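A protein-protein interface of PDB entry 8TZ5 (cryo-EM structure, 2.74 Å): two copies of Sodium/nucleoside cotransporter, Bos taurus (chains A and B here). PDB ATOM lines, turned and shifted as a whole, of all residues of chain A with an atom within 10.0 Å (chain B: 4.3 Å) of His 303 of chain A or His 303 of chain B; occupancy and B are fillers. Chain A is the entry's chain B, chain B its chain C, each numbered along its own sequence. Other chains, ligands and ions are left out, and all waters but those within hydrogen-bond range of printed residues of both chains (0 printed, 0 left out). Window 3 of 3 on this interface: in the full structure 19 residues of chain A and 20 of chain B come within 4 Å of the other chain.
The backbone NH (N) of Ala 306 of chain B sits close to the backbone carbonyl oxygen (O) of Val 295 of chain A (3.4 Å). ND1 of His 303 of chain B is in hydrogen-bond range of O of Phe 296 of chain A (2.9 Å). NE2 of His 303 of chain A is in hydrogen-bond range of NE2 of His 303 of chain B (3.5 Å).
Among the printed residues, merely in contact across the chains: Phe 294 of chain A with Phe 305 of chain B (3.6 Å), Val 295 of chain A with Phe 305 of chain B (3.8 Å), Lys 299 of chain A with Asp 302 of chain B (3.6 Å) and Lys 299 of chain A with His 303 of chain B (3.5 Å).
His 303 of chain A touches one residue of chain B. His 303 of chain B touches just these residues of chain A: Phe 296 (2.9 Å), Lys 299 (3.5 Å) and His 303 (3.5 Å). Of chain A, only Lys 299 comes within 4 Å of Asp 302 of chain B. Ala 306 of chain B touches just one residue of chain A: Val 295 (3.2 Å). No residue of chain A comes within 4 Å of Phe 307 of chain B. Printed residues of chain B within 4 Å of Phe 294 of chain A: Phe 305. Printed residues of chain A within 4 Å of Phe 305 of chain B: Phe 294 (3.6 Å) and Val 295 (3.8 Å). Printed residues of chain B within 4 Å of Lys 299 of chain A: Asp 302 (3.6 Å) and His 303 (3.5 Å). Printed residues of chain B within 4 Å of Val 295 of chain A: Phe 305 (3.8 Å) and Ala 306 (3.2 Å). Printed residues of chain B within 4 Å of Phe 296 of chain A: His 303. The nearest printed residue of chain B that does not touch His 303 of chain A is Phe 307 of chain B (5.9 Å).
Of the 9 printed residues of chain B, 4 touch a printed residue of chain A. Printed residues of chain B that touch a printed residue of chain A: Asp 302, His 303, Phe 305 and Ala 306. Among the printed residues, 7 pairs touch across the chains. Among the printed residues, no Asp or Glu carboxylate lies within 4 Å of a Lys or Arg side-chain nitrogen of the other chain.
His 303 of chain A touches its own counterpart, His 303 of chain B. Positions printed for both chains: 300, 301, 302, 303, 304, 305, 306, 307 and 308. Of the 7 pairs that touch across the chains among the printed residues, 1 has its exchanged pair printed and touching as well.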
ATOM      1  N   ALA A 292      -7.796  -5.904 -28.126  1.00  0.00           N
ATOM      2  CA  ALA A 292      -6.452  -6.208 -28.602  1.00  0.00           C
ATOM      3  C   ALA A 292      -5.386  -5.487 -27.786  1.00  0.00           C
ATOM      4  O   ALA A 292      -4.277  -6.007 -27.622  1.00  0.00           O
ATOM      5  CB  ALA A 292      -6.325  -5.843 -30.079  1.00  0.00           C
ATOM      6  N   SER A 293      -5.699  -4.297 -27.269  1.00  0.00           N
ATOM      7  CA  SER A 293      -4.747  -3.541 -26.470  1.00  0.00           C
ATOM      8  C   SER A 293      -4.604  -4.085 -25.057  1.00  0.00           C
ATOM      9  O   SER A 293      -3.596  -3.805 -24.402  1.00  0.00           O
ATOM     10  CB  SER A 293      -5.173  -2.073 -26.411  1.00  0.00           C
ATOM     11  OG  SER A 293      -4.219  -1.290 -25.717  1.00  0.00           O
ATOM     12  N   PHE A 294      -5.585  -4.843 -24.570  1.00  0.00           N
ATOM     13  CA  PHE A 294      -5.478  -5.455 -23.253  1.00  0.00           C
ATOM     14  C   PHE A 294      -4.856  -6.843 -23.324  1.00  0.00           C
ATOM     15  O   PHE A 294      -3.954  -7.160 -22.543  1.00  0.00           O
ATOM     16  CB  PHE A 294      -6.853  -5.532 -22.586  1.00  0.00           C
ATOM     17  CG  PHE A 294      -6.857  -6.327 -21.313  1.00  0.00           C
ATOM     18  CD1 PHE A 294      -6.176  -5.873 -20.196  1.00  0.00           C
ATOM     19  CD2 PHE A 294      -7.535  -7.531 -21.234  1.00  0.00           C
ATOM     20  CE1 PHE A 294      -6.172  -6.603 -19.027  1.00  0.00           C
ATOM     21  CE2 PHE A 294      -7.535  -8.265 -20.065  1.00  0.00           C
ATOM     22  CZ  PHE A 294      -6.853  -7.801 -18.960  1.00  0.00           C
ATOM     23  N   VAL A 295      -5.320  -7.682 -24.251  1.00  0.00           N
ATOM     24  CA  VAL A 295      -4.775  -9.032 -24.344  1.00  0.00           C
ATOM     25  C   VAL A 295      -3.320  -8.997 -24.793  1.00  0.00           C
ATOM     26  O   VAL A 295      -2.495  -9.792 -24.327  1.00  0.00           O
ATOM     27  CB  VAL A 295      -5.637  -9.898 -25.279  1.00  0.00           C
ATOM     28  CG1 VAL A 295      -4.960 -11.237 -25.531  1.00  0.00           C
ATOM     29  CG2 VAL A 295      -7.020 -10.095 -24.682  1.00  0.00           C
ATOM     30  N   PHE A 296      -2.979  -8.081 -25.698  1.00  0.00           N
ATOM     31  CA  PHE A 296      -1.633  -7.995 -26.248  1.00  0.00           C
ATOM     32  C   PHE A 296      -0.889  -6.732 -25.834  1.00  0.00           C
ATOM     33  O   PHE A 296       0.280  -6.574 -26.200  1.00  0.00           O
ATOM     34  CB  PHE A 296      -1.688  -8.088 -27.776  1.00  0.00           C
ATOM     35  CG  PHE A 296      -2.302  -9.362 -28.279  1.00  0.00           C
ATOM     36  CD1 PHE A 296      -1.712 -10.584 -28.009  1.00  0.00           C
ATOM     37  CD2 PHE A 296      -3.464  -9.339 -29.028  1.00  0.00           C
ATOM     38  CE1 PHE A 296      -2.273 -11.754 -28.469  1.00  0.00           C
ATOM     39  CE2 PHE A 296      -4.027 -10.509 -29.491  1.00  0.00           C
ATOM     40  CZ  PHE A 296      -3.429 -11.716 -29.211  1.00  0.00           C
ATOM     41  N   GLY A 297      -1.524  -5.833 -25.088  1.00  0.00           N
ATOM     42  CA  GLY A 297      -0.856  -4.658 -24.573  1.00  0.00           C
ATOM     43  C   GLY A 297      -0.870  -3.490 -25.542  1.00  0.00           C
ATOM     44  O   GLY A 297      -1.323  -3.580 -26.685  1.00  0.00           O
ATOM     45  N   GLU A 298      -0.354  -2.357 -25.056  1.00  0.00           N
ATOM     46  CA  GLU A 298      -0.263  -1.162 -25.887  1.00  0.00           C
ATOM     47  C   GLU A 298       0.676  -1.354 -27.068  1.00  0.00           C
ATOM     48  O   GLU A 298       0.576  -0.614 -28.053  1.00  0.00           O
ATOM     49  CB  GLU A 298       0.201   0.028 -25.047  1.00  0.00           C
ATOM     50  CG  GLU A 298      -0.780   0.440 -23.964  1.00  0.00           C
ATOM     51  CD  GLU A 298      -0.303   1.641 -23.171  1.00  0.00           C
ATOM     52  OE1 GLU A 298       0.809   2.136 -23.447  1.00  0.00           O
ATOM     53  OE2 GLU A 298      -1.043   2.093 -22.271  1.00  0.00           O
ATOM     54  N   LYS A 299       1.586  -2.325 -26.994  1.00  0.00           N
ATOM     55  CA  LYS A 299       2.503  -2.631 -28.081  1.00  0.00           C
ATOM     56  C   LYS A 299       1.922  -3.639 -29.066  1.00  0.00           C
ATOM     57  O   LYS A 299       2.679  -4.268 -29.814  1.00  0.00           O
ATOM     58  CB  LYS A 299       3.826  -3.150 -27.519  1.00  0.00           C
ATOM     59  CG  LYS A 299       4.653  -2.098 -26.805  1.00  0.00           C
ATOM     60  CD  LYS A 299       5.946  -2.687 -26.272  1.00  0.00           C
ATOM     61  CE  LYS A 299       6.854  -1.618 -25.694  1.00  0.00           C
ATOM     62  NZ  LYS A 299       7.298  -0.646 -26.728  1.00  0.00           N
ATOM     63  N   TYR A 300       0.599  -3.809 -29.078  1.00  0.00           N
ATOM     64  CA  TYR A 300      -0.024  -4.739 -30.011  1.00  0.00           C
ATOM     65  C   TYR A 300       0.181  -4.318 -31.460  1.00  0.00           C
ATOM     66  O   TYR A 300       0.021  -5.147 -32.363  1.00  0.00           O
ATOM     67  CB  TYR A 300      -1.518  -4.869 -29.702  1.00  0.00           C
ATOM     68  CG  TYR A 300      -2.346  -3.655 -30.060  1.00  0.00           C
ATOM     69  CD1 TYR A 300      -2.227  -2.470 -29.347  1.00  0.00           C
ATOM     70  CD2 TYR A 300      -3.264  -3.700 -31.100  1.00  0.00           C
ATOM     71  CE1 TYR A 300      -2.986  -1.364 -29.669  1.00  0.00           C
ATOM     72  CE2 TYR A 300      -4.028  -2.598 -31.427  1.00  0.00           C
ATOM     73  CZ  TYR A 300      -3.885  -1.434 -30.708  1.00  0.00           C
ATOM     74  OH  TYR A 300      -4.645  -0.334 -31.033  1.00  0.00           O
ATOM     75  N   THR A 301       0.534  -3.056 -31.703  1.00  0.00           N
ATOM     76  CA  THR A 301       0.803  -2.580 -33.051  1.00  0.00           C
ATOM     77  C   THR A 301       2.183  -2.976 -33.556  1.00  0.00           C
ATOM     78  O   THR A 301       2.444  -2.849 -34.757  1.00  0.00           O
ATOM     79  CB  THR A 301       0.658  -1.059 -33.105  1.00  0.00           C
ATOM     80  OG1 THR A 301       1.372  -0.469 -32.012  1.00  0.00           O
ATOM     81  CG2 THR A 301      -0.802  -0.662 -33.028  1.00  0.00           C
ATOM     82  N   ASP A 302       3.069  -3.450 -32.676  1.00  0.00           N
ATOM     83  CA  ASP A 302       4.364  -3.946 -33.121  1.00  0.00           C
ATOM     84  C   ASP A 302       4.224  -5.168 -34.017  1.00  0.00           C
ATOM     85  O   ASP A 302       5.120  -5.442 -34.821  1.00  0.00           O
ATOM     86  CB  ASP A 302       5.238  -4.284 -31.914  1.00  0.00           C
ATOM     87  CG  ASP A 302       5.608  -3.060 -31.102  1.00  0.00           C
ATOM     88  OD1 ASP A 302       5.171  -1.948 -31.465  1.00  0.00           O
ATOM     89  OD2 ASP A 302       6.337  -3.211 -30.099  1.00  0.00           O
ATOM     90  N   HIS A 303       3.120  -5.903 -33.891  1.00  0.00           N
ATOM     91  CA  HIS A 303       2.800  -7.041 -34.752  1.00  0.00           C
ATOM     92  C   HIS A 303       1.421  -6.739 -35.327  1.00  0.00           C
ATOM     93  O   HIS A 303       0.400  -7.138 -34.760  1.00  0.00           O
ATOM     94  CB  HIS A 303       2.826  -8.351 -33.976  1.00  0.00           C
ATOM     95  CG  HIS A 303       3.995  -8.480 -33.049  1.00  0.00           C
ATOM     96  ND1 HIS A 303       5.264  -8.789 -33.488  1.00  0.00           N
ATOM     97  CD2 HIS A 303       4.085  -8.340 -31.706  1.00  0.00           C
ATOM     98  CE1 HIS A 303       6.086  -8.834 -32.455  1.00  0.00           C
ATOM     99  NE2 HIS A 303       5.395  -8.565 -31.362  1.00  0.00           N
ATOM    100  N   PHE A 304       1.396  -6.030 -36.455  1.00  0.00           N
ATOM    101  CA  PHE A 304       0.142  -5.477 -36.955  1.00  0.00           C
ATOM    102  C   PHE A 304      -0.853  -6.580 -37.290  1.00  0.00           C
ATOM    103  O   PHE A 304      -1.956  -6.632 -36.735  1.00  0.00           O
ATOM    104  CB  PHE A 304       0.413  -4.600 -38.179  1.00  0.00           C
ATOM    105  CG  PHE A 304      -0.830  -4.047 -38.813  1.00  0.00           C
ATOM    106  CD1 PHE A 304      -1.471  -2.948 -38.271  1.00  0.00           C
ATOM    107  CD2 PHE A 304      -1.356  -4.629 -39.953  1.00  0.00           C
ATOM    108  CE1 PHE A 304      -2.615  -2.440 -38.854  1.00  0.00           C
ATOM    109  CE2 PHE A 304      -2.499  -4.126 -40.539  1.00  0.00           C
ATOM    110  CZ  PHE A 304      -3.129  -3.029 -39.989  1.00  0.00           C
ATOM    111  N   PHE A 305      -0.472  -7.492 -38.185  1.00  0.00           N
ATOM    112  CA  PHE A 305      -1.427  -8.477 -38.678  1.00  0.00           C
ATOM    113  C   PHE A 305      -1.978  -9.330 -37.542  1.00  0.00           C
ATOM    114  O   PHE A 305      -3.183  -9.315 -37.267  1.00  0.00           O
ATOM    115  CB  PHE A 305      -0.765  -9.355 -39.739  1.00  0.00           C
ATOM    116  CG  PHE A 305      -1.696 -10.349 -40.371  1.00  0.00           C
ATOM    117  CD1 PHE A 305      -2.608  -9.949 -41.329  1.00  0.00           C
ATOM    118  CD2 PHE A 305      -1.656 -11.685 -40.011  1.00  0.00           C
ATOM    119  CE1 PHE A 305      -3.464 -10.859 -41.912  1.00  0.00           C
ATOM    120  CE2 PHE A 305      -2.509 -12.598 -40.591  1.00  0.00           C
ATOM    121  CZ  PHE A 305      -3.415 -12.184 -41.543  1.00  0.00           C
ATOM    122  N   ALA A 306      -1.098 -10.040 -36.835  1.00  0.00           N
ATOM    123  CA  ALA A 306      -1.551 -11.055 -35.891  1.00  0.00           C
ATOM    124  C   ALA A 306      -2.349 -10.448 -34.746  1.00  0.00           C
ATOM    125  O   ALA A 306      -3.351 -11.026 -34.308  1.00  0.00           O
ATOM    126  CB  ALA A 306      -0.352 -11.829 -35.349  1.00  0.00           C
ATOM    127  N   PHE A 307      -1.927  -9.290 -34.247  1.00  0.00           N
ATOM    128  CA  PHE A 307      -2.488  -8.726 -33.030  1.00  0.00           C
ATOM    129  C   PHE A 307      -3.488  -7.604 -33.274  1.00  0.00           C
ATOM    130  O   PHE A 307      -4.023  -7.060 -32.303  1.00  0.00           O
ATOM    131  CB  PHE A 307      -1.359  -8.212 -32.127  1.00  0.00           C
ATOM    132  CG  PHE A 307      -0.488  -9.299 -31.543  1.00  0.00           C
ATOM    133  CD1 PHE A 307      -0.749 -10.640 -31.780  1.00  0.00           C
ATOM    134  CD2 PHE A 307       0.592  -8.971 -30.743  1.00  0.00           C
ATOM    135  CE1 PHE A 307       0.053 -11.622 -31.237  1.00  0.00           C
ATOM    136  CE2 PHE A 307       1.393  -9.952 -30.200  1.00  0.00           C
ATOM    137  CZ  PHE A 307       1.123 -11.275 -30.446  1.00  0.00           C
ATOM    138  N   LYS A 308      -3.761  -7.238 -34.529  1.00  0.00           N
ATOM    139  CA  LYS A 308      -4.751  -6.200 -34.795  1.00  0.00           C
ATOM    140  C   LYS A 308      -5.789  -6.636 -35.824  1.00  0.00           C
ATOM    141  O   LYS A 308      -6.946  -6.214 -35.750  1.00  0.00           O
ATOM    142  CB  LYS A 308      -4.061  -4.915 -35.258  1.00  0.00           C
ATOM    143  CG  LYS A 308      -5.019  -3.796 -35.612  1.00  0.00           C
ATOM    144  CD  LYS A 308      -4.399  -2.429 -35.383  1.00  0.00           C
ATOM    145  CE  LYS A 308      -5.338  -1.314 -35.818  1.00  0.00           C
ATOM    146  NZ  LYS A 308      -4.959   0.004 -35.239  1.00  0.00           N
ATOM    147  N   VAL A 309      -5.398  -7.472 -36.784  1.00  0.00           N
ATOM    148  CA  VAL A 309      -6.284  -7.814 -37.893  1.00  0.00           C
ATOM    149  C   VAL A 309      -7.149  -9.027 -37.571  1.00  0.00           C
ATOM    150  O   VAL A 309      -8.333  -9.058 -37.913  1.00  0.00           O
ATOM    151  CB  VAL A 309      -5.450  -8.038 -39.168  1.00  0.00           C
ATOM    152  CG1 VAL A 309      -6.328  -8.530 -40.302  1.00  0.00           C
ATOM    153  CG2 VAL A 309      -4.740  -6.756 -39.562  1.00  0.00           C
ATOM    154  N   LEU A 310      -6.582 -10.043 -36.929  1.00  0.00           N
ATOM    155  CA  LEU A 310      -7.325 -11.252 -36.589  1.00  0.00           C
ATOM    156  C   LEU A 310      -8.361 -10.973 -35.503  1.00  0.00           C
ATOM    157  O   LEU A 310      -9.449 -11.567 -35.521  1.00  0.00           O
ATOM    158  CB  LEU A 310      -6.362 -12.355 -36.151  1.00  0.00           C
ATOM    159  CG  LEU A 310      -5.353 -12.794 -37.216  1.00  0.00           C
ATOM    160  CD1 LEU A 310      -4.385 -13.814 -36.649  1.00  0.00           C
ATOM    161  CD2 LEU A 310      -6.056 -13.352 -38.447  1.00  0.00           C
ATOM    162  N   PRO A 311      -8.070 -10.097 -34.535  1.00  0.00           N
ATOM    163  CA  PRO A 311      -9.129  -9.687 -33.602  1.00  0.00           C
ATOM    164  C   PRO A 311     -10.336  -9.091 -34.299  1.00  0.00           C
ATOM    165  O   PRO A 311     -11.463  -9.245 -33.811  1.00  0.00           O
ATOM    166  CB  PRO A 311      -8.421  -8.663 -32.707  1.00  0.00           C
ATOM    167  CG  PRO A 311      -7.009  -9.096 -32.709  1.00  0.00           C
ATOM    168  CD  PRO A 311      -6.743  -9.642 -34.082  1.00  0.00           C
ATOM    169  N   TYR B 300       9.393 -10.503 -23.221  1.00  0.00           N
ATOM    170  CA  TYR B 300       8.065 -11.033 -22.939  1.00  0.00           C
ATOM    171  C   TYR B 300       7.231 -10.072 -22.103  1.00  0.00           C
ATOM    172  O   TYR B 300       6.004 -10.207 -22.063  1.00  0.00           O
ATOM    173  CB  TYR B 300       8.180 -12.388 -22.235  1.00  0.00           C
ATOM    174  CG  TYR B 300       8.666 -12.319 -20.803  1.00  0.00           C
ATOM    175  CD1 TYR B 300       9.977 -11.971 -20.507  1.00  0.00           C
ATOM    176  CD2 TYR B 300       7.818 -12.622 -19.748  1.00  0.00           C
ATOM    177  CE1 TYR B 300      10.422 -11.913 -19.203  1.00  0.00           C
ATOM    178  CE2 TYR B 300       8.256 -12.567 -18.442  1.00  0.00           C
ATOM    179  CZ  TYR B 300       9.558 -12.213 -18.175  1.00  0.00           C
ATOM    180  OH  TYR B 300       9.998 -12.158 -16.873  1.00  0.00           O
ATOM    181  N   THR B 301       7.867  -9.107 -21.438  1.00  0.00           N
ATOM    182  CA  THR B 301       7.146  -8.114 -20.655  1.00  0.00           C
ATOM    183  C   THR B 301       6.540  -7.010 -21.513  1.00  0.00           C
ATOM    184  O   THR B 301       5.710  -6.246 -21.010  1.00  0.00           O
ATOM    185  CB  THR B 301       8.079  -7.494 -19.614  1.00  0.00           C
ATOM    186  OG1 THR B 301       9.313  -7.118 -20.237  1.00  0.00           O
ATOM    187  CG2 THR B 301       8.356  -8.481 -18.497  1.00  0.00           C
ATOM    188  N   ASP B 302       6.932  -6.909 -22.784  1.00  0.00           N
ATOM    189  CA  ASP B 302       6.305  -5.943 -23.678  1.00  0.00           C
ATOM    190  C   ASP B 302       4.831  -6.248 -23.895  1.00  0.00           C
ATOM    191  O   ASP B 302       4.061  -5.341 -24.227  1.00  0.00           O
ATOM    192  CB  ASP B 302       7.035  -5.923 -25.021  1.00  0.00           C
ATOM    193  CG  ASP B 302       8.452  -5.402 -24.907  1.00  0.00           C
ATOM    194  OD1 ASP B 302       8.878  -5.073 -23.779  1.00  0.00           O
ATOM    195  OD2 ASP B 302       9.141  -5.322 -25.945  1.00  0.00           O
ATOM    196  N   HIS B 303       4.426  -7.504 -23.713  1.00  0.00           N
ATOM    197  CA  HIS B 303       3.028  -7.926 -23.783  1.00  0.00           C
ATOM    198  C   HIS B 303       2.746  -8.621 -22.456  1.00  0.00           C
ATOM    199  O   HIS B 303       2.898  -9.839 -22.338  1.00  0.00           O
ATOM    200  CB  HIS B 303       2.780  -8.840 -24.976  1.00  0.00           C
ATOM    201  CG  HIS B 303       3.436  -8.376 -26.238  1.00  0.00           C
ATOM    202  ND1 HIS B 303       2.933  -7.347 -27.005  1.00  0.00           N
ATOM    203  CD2 HIS B 303       4.557  -8.801 -26.867  1.00  0.00           C
ATOM    204  CE1 HIS B 303       3.716  -7.157 -28.052  1.00  0.00           C
ATOM    205  NE2 HIS B 303       4.709  -8.026 -27.992  1.00  0.00           N
ATOM    206  N   PHE B 304       2.337  -7.839 -21.456  1.00  0.00           N
ATOM    207  CA  PHE B 304       2.279  -8.352 -20.091  1.00  0.00           C
ATOM    208  C   PHE B 304       1.288  -9.502 -19.975  1.00  0.00           C
ATOM    209  O   PHE B 304       1.653 -10.617 -19.589  1.00  0.00           O
ATOM    210  CB  PHE B 304       1.913  -7.220 -19.129  1.00  0.00           C
ATOM    211  CG  PHE B 304       1.751  -7.667 -17.706  1.00  0.00           C
ATOM    212  CD1 PHE B 304       2.856  -7.880 -16.901  1.00  0.00           C
ATOM    213  CD2 PHE B 304       0.491  -7.873 -17.172  1.00  0.00           C
ATOM    214  CE1 PHE B 304       2.708  -8.293 -15.593  1.00  0.00           C
ATOM    215  CE2 PHE B 304       0.337  -8.285 -15.864  1.00  0.00           C
ATOM    216  CZ  PHE B 304       1.446  -8.495 -15.074  1.00  0.00           C
ATOM    217  N   PHE B 305       0.027  -9.256 -20.330  1.00  0.00           N
ATOM    218  CA  PHE B 305      -1.008 -10.254 -20.091  1.00  0.00           C
ATOM    219  C   PHE B 305      -0.701 -11.556 -20.821  1.00  0.00           C
ATOM    220  O   PHE B 305      -0.510 -12.603 -20.192  1.00  0.00           O
ATOM    221  CB  PHE B 305      -2.369  -9.705 -20.518  1.00  0.00           C
ATOM    222  CG  PHE B 305      -3.515 -10.630 -20.231  1.00  0.00           C
ATOM    223  CD1 PHE B 305      -4.014 -10.756 -18.949  1.00  0.00           C
ATOM    224  CD2 PHE B 305      -4.097 -11.373 -21.245  1.00  0.00           C
ATOM    225  CE1 PHE B 305      -5.067 -11.604 -18.680  1.00  0.00           C
ATOM    226  CE2 PHE B 305      -5.150 -12.222 -20.980  1.00  0.00           C
ATOM    227  CZ  PHE B 305      -5.635 -12.338 -19.697  1.00  0.00           C
ATOM    228  N   ALA B 306      -0.593 -11.495 -22.149  1.00  0.00           N
ATOM    229  CA  ALA B 306      -0.536 -12.716 -22.944  1.00  0.00           C
ATOM    230  C   ALA B 306       0.712 -13.533 -22.637  1.00  0.00           C
ATOM    231  O   ALA B 306       0.651 -14.767 -22.576  1.00  0.00           O
ATOM    232  CB  ALA B 306      -0.588 -12.369 -24.429  1.00  0.00           C
ATOM    233  N   PHE B 307       1.849 -12.872 -22.441  1.00  0.00           N
ATOM    234  CA  PHE B 307       3.129 -13.554 -22.344  1.00  0.00           C
ATOM    235  C   PHE B 307       3.638 -13.709 -20.917  1.00  0.00           C
ATOM    236  O   PHE B 307       4.717 -14.279 -20.728  1.00  0.00           O
ATOM    237  CB  PHE B 307       4.180 -12.811 -23.180  1.00  0.00           C
ATOM    238  CG  PHE B 307       3.950 -12.883 -24.670  1.00  0.00           C
ATOM    239  CD1 PHE B 307       2.900 -13.613 -25.205  1.00  0.00           C
ATOM    240  CD2 PHE B 307       4.800 -12.221 -25.538  1.00  0.00           C
ATOM    241  CE1 PHE B 307       2.704 -13.671 -26.570  1.00  0.00           C
ATOM    242  CE2 PHE B 307       4.606 -12.280 -26.900  1.00  0.00           C
ATOM    243  CZ  PHE B 307       3.559 -13.004 -27.416  1.00  0.00           C
ATOM    244  N   LYS B 308       2.906 -13.228 -19.909  1.00  0.00           N
ATOM    245  CA  LYS B 308       3.344 -13.405 -18.529  1.00  0.00           C
ATOM    246  C   LYS B 308       2.250 -13.988 -17.642  1.00  0.00           C
ATOM    247  O   LYS B 308       2.549 -14.726 -16.697  1.00  0.00           O
ATOM    248  CB  LYS B 308       3.833 -12.075 -17.954  1.00  0.00           C
ATOM    249  CG  LYS B 308       4.257 -12.152 -16.500  1.00  0.00           C
ATOM    250  CD  LYS B 308       5.327 -11.127 -16.170  1.00  0.00           C
ATOM    251  CE  LYS B 308       5.686 -11.158 -14.692  1.00  0.00           C
ATOM    252  NZ  LYS B 308       6.987 -10.489 -14.411  1.00  0.00           N
